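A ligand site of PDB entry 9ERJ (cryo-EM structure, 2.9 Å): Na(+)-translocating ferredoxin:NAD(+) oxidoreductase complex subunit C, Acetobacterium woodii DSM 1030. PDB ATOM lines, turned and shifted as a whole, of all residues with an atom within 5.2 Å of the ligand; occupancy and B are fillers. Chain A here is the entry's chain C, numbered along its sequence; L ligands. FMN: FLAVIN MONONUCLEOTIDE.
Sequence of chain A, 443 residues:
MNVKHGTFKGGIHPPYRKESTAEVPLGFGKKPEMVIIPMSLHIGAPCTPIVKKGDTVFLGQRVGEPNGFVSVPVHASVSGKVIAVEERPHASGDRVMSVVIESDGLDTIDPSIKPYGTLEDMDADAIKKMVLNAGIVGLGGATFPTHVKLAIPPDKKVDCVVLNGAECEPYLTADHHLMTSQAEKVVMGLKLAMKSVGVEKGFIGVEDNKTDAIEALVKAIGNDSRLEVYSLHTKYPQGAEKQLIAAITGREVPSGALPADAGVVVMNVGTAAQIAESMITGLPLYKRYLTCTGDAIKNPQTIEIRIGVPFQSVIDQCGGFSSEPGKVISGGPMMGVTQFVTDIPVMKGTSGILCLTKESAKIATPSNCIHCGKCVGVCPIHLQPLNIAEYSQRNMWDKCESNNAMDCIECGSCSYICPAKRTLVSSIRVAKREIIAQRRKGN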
ATOM      1  N   GLY A 138     -16.975  -0.077  32.805  1.00  0.00           N
ATOM      2  CA  GLY A 138     -15.810   0.226  31.999  1.00  0.00           C
ATOM      3  C   GLY A 138     -15.023   1.388  32.573  1.00  0.00           C
ATOM      4  O   GLY A 138     -15.556   2.509  32.695  1.00  0.00           O
ATOM      5  N   LEU A 139     -13.765   1.152  32.928  1.00  0.00           N
ATOM      6  CA  LEU A 139     -12.905   2.193  33.488  1.00  0.00           C
ATOM      7  C   LEU A 139     -12.220   3.025  32.432  1.00  0.00           C
ATOM      8  O   LEU A 139     -11.455   3.933  32.776  1.00  0.00           O
ATOM      9  CB  LEU A 139     -11.853   1.573  34.412  1.00  0.00           C
ATOM     10  CG  LEU A 139     -12.312   0.748  35.622  1.00  0.00           C
ATOM     11  CD1 LEU A 139     -11.179   0.620  36.625  1.00  0.00           C
ATOM     12  CD2 LEU A 139     -13.532   1.371  36.283  1.00  0.00           C
ATOM     13  N   GLY A 140     -12.466   2.758  31.149  1.00  0.00           N
ATOM     14  CA  GLY A 140     -11.828   3.525  30.083  1.00  0.00           C
ATOM     15  C   GLY A 140     -12.393   4.910  29.900  1.00  0.00           C
ATOM     16  O   GLY A 140     -11.739   5.754  29.277  1.00  0.00           O
ATOM     17  N   ALA A 142     -16.126   5.497  29.262  1.00  0.00           N
ATOM     18  CA  ALA A 142     -17.521   5.444  28.845  1.00  0.00           C
ATOM     19  C   ALA A 142     -18.441   4.856  29.898  1.00  0.00           C
ATOM     20  O   ALA A 142     -19.642   5.144  29.871  1.00  0.00           O
ATOM     21  CB  ALA A 142     -17.648   4.628  27.546  1.00  0.00           C
ATOM     22  N   THR A 143     -17.907   4.054  30.822  1.00  0.00           N
ATOM     23  CA  THR A 143     -18.662   3.430  31.920  1.00  0.00           C
ATOM     24  C   THR A 143     -19.856   2.629  31.412  1.00  0.00           C
ATOM     25  O   THR A 143     -20.988   2.770  31.882  1.00  0.00           O
ATOM     26  CB  THR A 143     -19.106   4.463  32.964  1.00  0.00           C
ATOM     27  OG1 THR A 143     -20.000   5.415  32.371  1.00  0.00           O
ATOM     28  CG2 THR A 143     -17.901   5.191  33.532  1.00  0.00           C
ATOM     29  N   PHE A 144     -19.594   1.772  30.427  1.00  0.00           N
ATOM     30  CA  PHE A 144     -20.571   0.793  29.959  1.00  0.00           C
ATOM     31  C   PHE A 144     -20.460  -0.483  30.796  1.00  0.00           C
ATOM     32  O   PHE A 144     -19.351  -0.895  31.138  1.00  0.00           O
ATOM     33  CB  PHE A 144     -20.342   0.464  28.488  1.00  0.00           C
ATOM     34  CG  PHE A 144     -21.454  -0.331  27.854  1.00  0.00           C
ATOM     35  CD1 PHE A 144     -22.640   0.287  27.490  1.00  0.00           C
ATOM     36  CD2 PHE A 144     -21.304  -1.684  27.628  1.00  0.00           C
ATOM     37  CE1 PHE A 144     -23.662  -0.441  26.911  1.00  0.00           C
ATOM     38  CE2 PHE A 144     -22.326  -2.413  27.049  1.00  0.00           C
ATOM     39  CZ  PHE A 144     -23.500  -1.798  26.692  1.00  0.00           C
ATOM     40  N   LYS A 149     -21.355  -6.554  28.025  1.00  0.00           N
ATOM     41  CA  LYS A 149     -20.353  -6.682  26.974  1.00  0.00           C
ATOM     42  C   LYS A 149     -19.920  -8.126  26.781  1.00  0.00           C
ATOM     43  O   LYS A 149     -19.630  -8.542  25.644  1.00  0.00           O
ATOM     44  CB  LYS A 149     -19.151  -5.795  27.293  1.00  0.00           C
ATOM     45  CG  LYS A 149     -18.131  -5.686  26.177  1.00  0.00           C
ATOM     46  CD  LYS A 149     -16.750  -5.408  26.726  1.00  0.00           C
ATOM     47  CE  LYS A 149     -16.553  -3.923  26.987  1.00  0.00           C
ATOM     48  NZ  LYS A 149     -16.774  -3.114  25.753  1.00  0.00           N
ATOM     49  N   ASN A 164      -6.627  -2.462  25.822  1.00  0.00           N
ATOM     50  CA  ASN A 164      -6.250  -1.117  25.410  1.00  0.00           C
ATOM     51  C   ASN A 164      -5.287  -0.533  26.431  1.00  0.00           C
ATOM     52  O   ASN A 164      -5.696   0.044  27.434  1.00  0.00           O
ATOM     53  CB  ASN A 164      -7.490  -0.238  25.254  1.00  0.00           C
ATOM     54  CG  ASN A 164      -7.287   0.914  24.301  1.00  0.00           C
ATOM     55  OD1 ASN A 164      -6.180   1.441  24.177  1.00  0.00           O
ATOM     56  ND2 ASN A 164      -8.342   1.306  23.615  1.00  0.00           N
ATOM     57  N   ALA A 166      -2.889   1.672  25.279  1.00  0.00           N
ATOM     58  CA  ALA A 166      -2.335   2.842  24.594  1.00  0.00           C
ATOM     59  C   ALA A 166      -2.957   4.112  25.175  1.00  0.00           C
ATOM     60  O   ALA A 166      -3.773   4.790  24.548  1.00  0.00           O
ATOM     61  CB  ALA A 166      -2.564   2.740  23.102  1.00  0.00           C
ATOM     62  N   GLU A 167      -2.547   4.426  26.402  1.00  0.00           N
ATOM     63  CA  GLU A 167      -2.979   5.662  27.045  1.00  0.00           C
ATOM     64  C   GLU A 167      -2.324   6.842  26.350  1.00  0.00           C
ATOM     65  O   GLU A 167      -1.102   6.967  26.324  1.00  0.00           O
ATOM     66  CB  GLU A 167      -2.618   5.623  28.523  1.00  0.00           C
ATOM     67  CG  GLU A 167      -2.698   6.962  29.224  1.00  0.00           C
ATOM     68  CD  GLU A 167      -2.312   6.871  30.689  1.00  0.00           C
ATOM     69  OE1 GLU A 167      -1.126   6.602  30.974  1.00  0.00           O
ATOM     70  OE2 GLU A 167      -3.195   7.062  31.548  1.00  0.00           O
ATOM     71  N   CYS A 168      -3.144   7.725  25.780  1.00  0.00           N
ATOM     72  CA  CYS A 168      -2.679   8.691  24.800  1.00  0.00           C
ATOM     73  C   CYS A 168      -2.921  10.150  25.169  1.00  0.00           C
ATOM     74  O   CYS A 168      -2.288  11.031  24.574  1.00  0.00           O
ATOM     75  CB  CYS A 168      -3.319   8.417  23.437  1.00  0.00           C
ATOM     76  SG  CYS A 168      -5.102   8.163  23.521  1.00  0.00           S
ATOM     77  N   GLU A 169      -3.806  10.442  26.116  1.00  0.00           N
ATOM     78  CA  GLU A 169      -4.062  11.831  26.444  1.00  0.00           C
ATOM     79  C   GLU A 169      -2.906  12.410  27.255  1.00  0.00           C
ATOM     80  O   GLU A 169      -2.292  11.715  28.066  1.00  0.00           O
ATOM     81  CB  GLU A 169      -5.362  11.976  27.226  1.00  0.00           C
ATOM     82  CG  GLU A 169      -6.582  11.532  26.453  1.00  0.00           C
ATOM     83  CD  GLU A 169      -7.692  12.558  26.487  1.00  0.00           C
ATOM     84  OE1 GLU A 169      -7.518  13.597  27.157  1.00  0.00           O
ATOM     85  OE2 GLU A 169      -8.732  12.336  25.842  1.00  0.00           O
ATOM     86  N   ASP A 175      -2.245   4.644  33.922  1.00  0.00           N
ATOM     87  CA  ASP A 175      -2.104   3.327  33.333  1.00  0.00           C
ATOM     88  C   ASP A 175      -0.647   2.883  33.268  1.00  0.00           C
ATOM     89  O   ASP A 175      -0.365   1.682  33.353  1.00  0.00           O
ATOM     90  CB  ASP A 175      -2.719   3.305  31.928  1.00  0.00           C
ATOM     91  CG  ASP A 175      -4.209   3.027  31.956  1.00  0.00           C
ATOM     92  OD1 ASP A 175      -4.820   3.145  33.039  1.00  0.00           O
ATOM     93  OD2 ASP A 175      -4.766   2.708  30.882  1.00  0.00           O
ATOM     94  N   TYR A 236      -2.078  10.785  19.029  1.00  0.00           N
ATOM     95  CA  TYR A 236      -3.161  11.118  19.961  1.00  0.00           C
ATOM     96  C   TYR A 236      -4.387  10.210  19.793  1.00  0.00           C
ATOM     97  O   TYR A 236      -4.779   9.557  20.783  1.00  0.00           O
ATOM     98  CB  TYR A 236      -3.513  12.607  19.859  1.00  0.00           C
ATOM     99  CG  TYR A 236      -4.930  12.909  20.310  1.00  0.00           C
ATOM    100  CD1 TYR A 236      -5.321  12.736  21.633  1.00  0.00           C
ATOM    101  CD2 TYR A 236      -5.873  13.372  19.404  1.00  0.00           C
ATOM    102  CE1 TYR A 236      -6.607  13.001  22.040  1.00  0.00           C
ATOM    103  CE2 TYR A 236      -7.170  13.650  19.808  1.00  0.00           C
ATOM    104  CZ  TYR A 236      -7.521  13.462  21.127  1.00  0.00           C
ATOM    105  OH  TYR A 236      -8.808  13.740  21.528  1.00  0.00           O
ATOM    106  N   GLY A 239      -5.665   5.387  20.597  1.00  0.00           N
ATOM    107  CA  GLY A 239      -6.332   4.481  21.505  1.00  0.00           C
ATOM    108  C   GLY A 239      -7.840   4.475  21.476  1.00  0.00           C
ATOM    109  O   GLY A 239      -8.452   3.928  22.393  1.00  0.00           O
ATOM    110  N   ALA A 240      -8.482   5.065  20.465  1.00  0.00           N
ATOM    111  CA  ALA A 240      -9.940   5.220  20.477  1.00  0.00           C
ATOM    112  C   ALA A 240     -10.678   4.019  19.900  1.00  0.00           C
ATOM    113  O   ALA A 240     -11.576   4.200  19.073  1.00  0.00           O
ATOM    114  CB  ALA A 240     -10.318   6.495  19.726  1.00  0.00           C
ATOM    115  N   GLU A 241     -10.300   2.801  20.280  1.00  0.00           N
ATOM    116  CA  GLU A 241     -11.089   1.569  20.115  1.00  0.00           C
ATOM    117  C   GLU A 241     -11.307   1.185  18.646  1.00  0.00           C
ATOM    118  O   GLU A 241     -11.750   0.071  18.351  1.00  0.00           O
ATOM    119  CB  GLU A 241     -12.437   1.709  20.831  1.00  0.00           C
ATOM    120  CG  GLU A 241     -13.254   0.422  20.968  1.00  0.00           C
ATOM    121  CD  GLU A 241     -14.742   0.668  21.040  1.00  0.00           C
ATOM    122  OE1 GLU A 241     -15.314   1.150  20.041  1.00  0.00           O
ATOM    123  OE2 GLU A 241     -15.344   0.383  22.095  1.00  0.00           O
ATOM    124  N   VAL A 266     -13.025  -5.578  22.943  1.00  0.00           N
ATOM    125  CA  VAL A 266     -12.028  -4.613  23.413  1.00  0.00           C
ATOM    126  C   VAL A 266     -12.301  -4.285  24.873  1.00  0.00           C
ATOM    127  O   VAL A 266     -13.426  -3.903  25.238  1.00  0.00           O
ATOM    128  CB  VAL A 266     -12.050  -3.333  22.557  1.00  0.00           C
ATOM    129  CG1 VAL A 266     -10.988  -2.359  23.035  1.00  0.00           C
ATOM    130  CG2 VAL A 266     -11.841  -3.670  21.087  1.00  0.00           C
ATOM    131  N   MET A 267     -11.284  -4.434  25.714  1.00  0.00           N
ATOM    132  CA  MET A 267     -11.373  -4.130  27.133  1.00  0.00           C
ATOM    133  C   MET A 267     -10.193  -3.252  27.530  1.00  0.00           C
ATOM    134  O   MET A 267      -9.309  -2.954  26.724  1.00  0.00           O
ATOM    135  CB  MET A 267     -11.426  -5.406  27.976  1.00  0.00           C
ATOM    136  CG  MET A 267     -12.430  -5.357  29.120  1.00  0.00           C
ATOM    137  SD  MET A 267     -12.527  -6.885  30.052  1.00  0.00           S
ATOM    138  CE  MET A 267     -10.803  -7.135  30.451  1.00  0.00           C
ATOM    139  N   ASN A 268     -10.182  -2.830  28.791  1.00  0.00           N
ATOM    140  CA  ASN A 268      -9.148  -1.969  29.346  1.00  0.00           C
ATOM    141  C   ASN A 268      -8.288  -2.759  30.326  1.00  0.00           C
ATOM    142  O   ASN A 268      -8.700  -3.795  30.849  1.00  0.00           O
ATOM    143  CB  ASN A 268      -9.765  -0.754  30.038  1.00  0.00           C
ATOM    144  CG  ASN A 268      -8.816   0.429  30.116  1.00  0.00           C
ATOM    145  OD1 ASN A 268      -8.468   1.013  29.091  1.00  0.00           O
ATOM    146  ND2 ASN A 268      -8.398   0.768  31.327  1.00  0.00           N
ATOM    147  N   THR A 271      -9.822  -2.485  33.919  1.00  0.00           N
ATOM    148  CA  THR A 271     -10.944  -3.399  34.112  1.00  0.00           C
ATOM    149  C   THR A 271     -10.458  -4.823  34.356  1.00  0.00           C
ATOM    150  O   THR A 271     -11.003  -5.540  35.210  1.00  0.00           O
ATOM    151  CB  THR A 271     -11.876  -3.352  32.904  1.00  0.00           C
ATOM    152  OG1 THR A 271     -12.108  -1.990  32.536  1.00  0.00           O
ATOM    153  CG2 THR A 271     -13.214  -3.995  33.239  1.00  0.00           C
ATOM    154  N   MET A 335     -10.642  15.751  25.996  1.00  0.00           N
ATOM    155  CA  MET A 335     -12.022  15.294  26.047  1.00  0.00           C
ATOM    156  C   MET A 335     -12.660  15.490  27.410  1.00  0.00           C
ATOM    157  O   MET A 335     -13.736  14.932  27.657  1.00  0.00           O
ATOM    158  CB  MET A 335     -12.121  13.817  25.645  1.00  0.00           C
ATOM    159  CG  MET A 335     -12.193  13.580  24.147  1.00  0.00           C
ATOM    160  SD  MET A 335     -12.873  11.965  23.732  1.00  0.00           S
ATOM    161  CE  MET A 335     -14.599  12.371  23.449  1.00  0.00           C
ATOM    162  N   ILE A 409     -16.310  10.794  15.557  1.00  0.00           N
ATOM    163  CA  ILE A 409     -16.052  10.238  16.877  1.00  0.00           C
ATOM    164  C   ILE A 409     -15.799  11.323  17.922  1.00  0.00           C
ATOM    165  O   ILE A 409     -15.548  10.994  19.082  1.00  0.00           O
ATOM    166  CB  ILE A 409     -14.876   9.243  16.848  1.00  0.00           C
ATOM    167  CG1 ILE A 409     -13.651   9.878  16.203  1.00  0.00           C
ATOM    168  CG2 ILE A 409     -15.277   7.980  16.115  1.00  0.00           C
ATOM    169  CD1 ILE A 409     -12.360   9.155  16.517  1.00  0.00           C
ATOM    170  N   GLU A 410     -15.876  12.597  17.531  1.00  0.00           N
ATOM    171  CA  GLU A 410     -15.698  13.746  18.431  1.00  0.00           C
ATOM    172  C   GLU A 410     -14.353  13.669  19.163  1.00  0.00           C
ATOM    173  O   GLU A 410     -14.288  13.590  20.385  1.00  0.00           O
ATOM    174  CB  GLU A 410     -16.861  13.851  19.426  1.00  0.00           C
ATOM    175  CG  GLU A 410     -18.214  14.114  18.779  1.00  0.00           C
ATOM    176  CD  GLU A 410     -19.346  13.437  19.518  1.00  0.00           C
ATOM    177  OE1 GLU A 410     -19.164  13.082  20.697  1.00  0.00           O
ATOM    178  OE2 GLU A 410     -20.423  13.259  18.918  1.00  0.00           O
ATOM    179  N   CYS A 411     -13.269  13.711  18.387  1.00  0.00           N
ATOM    180  CA  CYS A 411     -11.938  13.523  18.934  1.00  0.00           C
ATOM    181  C   CYS A 411     -11.178  14.821  19.171  1.00  0.00           C
ATOM    182  O   CYS A 411     -10.103  14.791  19.767  1.00  0.00           O
ATOM    183  CB  CYS A 411     -11.114  12.611  18.012  1.00  0.00           C
ATOM    184  SG  CYS A 411     -10.614  13.365  16.456  1.00  0.00           S
HETATM  185  N1  FMN L   1      -9.890   4.243  26.225  1.00  0.00           N
HETATM  186  C2  FMN L   1      -8.757   3.926  26.874  1.00  0.00           C
HETATM  187  O2  FMN L   1      -8.719   2.966  27.638  1.00  0.00           O
HETATM  188  N3  FMN L   1      -7.607   4.637  26.715  1.00  0.00           N
HETATM  189  C4  FMN L   1      -7.541   5.729  25.883  1.00  0.00           C
HETATM  190  O4  FMN L   1      -6.490   6.335  25.767  1.00  0.00           O
HETATM  191  C4A FMN L   1      -8.705   6.097  25.183  1.00  0.00           C
HETATM  192  N5  FMN L   1      -8.664   7.128  24.391  1.00  0.00           N
HETATM  193  C5A FMN L   1      -9.812   7.465  23.719  1.00  0.00           C
HETATM  194  C6  FMN L   1      -9.773   8.580  22.858  1.00  0.00           C
HETATM  195  C7  FMN L   1     -10.884   8.974  22.154  1.00  0.00           C
HETATM  196  C7M FMN L   1     -10.814  10.165  21.235  1.00  0.00           C
HETATM  197  C8  FMN L   1     -12.099   8.254  22.304  1.00  0.00           C
HETATM  198  C8M FMN L   1     -13.328   8.660  21.545  1.00  0.00           C
HETATM  199  C9  FMN L   1     -12.140   7.164  23.152  1.00  0.00           C
HETATM  200  C9A FMN L   1     -11.017   6.744  23.867  1.00  0.00           C
HETATM  201  N10 FMN L   1     -11.022   5.644  24.735  1.00  0.00           N
HETATM  202  C10 FMN L   1      -9.874   5.285  25.410  1.00  0.00           C
HETATM  203  C1' FMN L   1     -12.251   4.861  24.922  1.00  0.00           C
HETATM  204  C2' FMN L   1     -12.369   3.720  23.935  1.00  0.00           C
HETATM  205  O2' FMN L   1     -12.926   4.203  22.716  1.00  0.00           O
HETATM  206  C3' FMN L   1     -13.237   2.582  24.479  1.00  0.00           C
HETATM  207  O3' FMN L   1     -14.506   3.095  24.857  1.00  0.00           O
HETATM  208  C4' FMN L   1     -12.602   1.838  25.657  1.00  0.00           C
HETATM  209  O4' FMN L   1     -11.455   1.117  25.218  1.00  0.00           O
HETATM  210  C5' FMN L   1     -13.569   0.895  26.333  1.00  0.00           C
HETATM  211  O5' FMN L   1     -12.974   0.366  27.550  1.00  0.00           O
HETATM  212  P   FMN L   1     -13.881  -0.539  28.527  1.00  0.00           P
HETATM  213  O1P FMN L   1     -14.236  -1.777  27.726  1.00  0.00           O
HETATM  214  O2P FMN L   1     -13.017  -0.838  29.732  1.00  0.00           O
HETATM  215  O3P FMN L   1     -15.079   0.315  28.860  1.00  0.00           O
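An oxygen (O2) of the ligand sits close to the side-chain amide oxygen (OD1) of Asn 268. OG1 of Thr 271 sits at hydrogen-bond distance from O2P of the ligand (3.2 Å). The side-chain sulfur (SG) of Cys 168 is in hydrogen-bond range of an oxygen (O4) of the ligand (3.2 Å). An oxygen (O1P) of the ligand is in salt-bridge range of the side-chain amino group (NZ) of Lys 149.
O of Ala 166 sits close to O4 of the ligand, 3.4 Å away. The backbone carbonyl oxygen (O) of Val 266 lies close to an oxygen (O1P) of the ligand. Merely in contact with the ligand: Glu 241, Gly 138, Asn 164, Ala 240, Gly 239, Met 335, Met 267, Glu 167, Leu 139 and Gly 140. Of the 25 residues printed, 16 come within 4 Å of the ligand. The nearest printed residue that does not touch the ligand is Ile 409 (4.1 Å).
The side-chain amide oxygen of Asn 268 lies close to the backbone carbonyl oxygen of Asn 164 (3.4 Å). SG of Cys 168 lies within hydrogen-bond range of O of Ala 166. O of Tyr 236 lies within hydrogen-bond range of SG of Cys 168, 3.1 Å away. N of Gly 138 sits at hydrogen-bond distance from O of Phe 144 (3.0 Å). The side-chain amino group of Lys 149 lies within hydrogen-bond range of the backbone carbonyl oxygen of Val 266 (3.5 Å). N of Ala 166 lies close to OD1 of Asn 164, at 3.5 Å. The side-chain amide nitrogen (ND2) of Asn 164 is in hydrogen-bond range of the backbone carbonyl oxygen (O) of Gly 239 (2.9 Å). The backbone NH (N) of Asn 164 lies within hydrogen-bond range of the backbone carbonyl oxygen (O) of Met 267.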
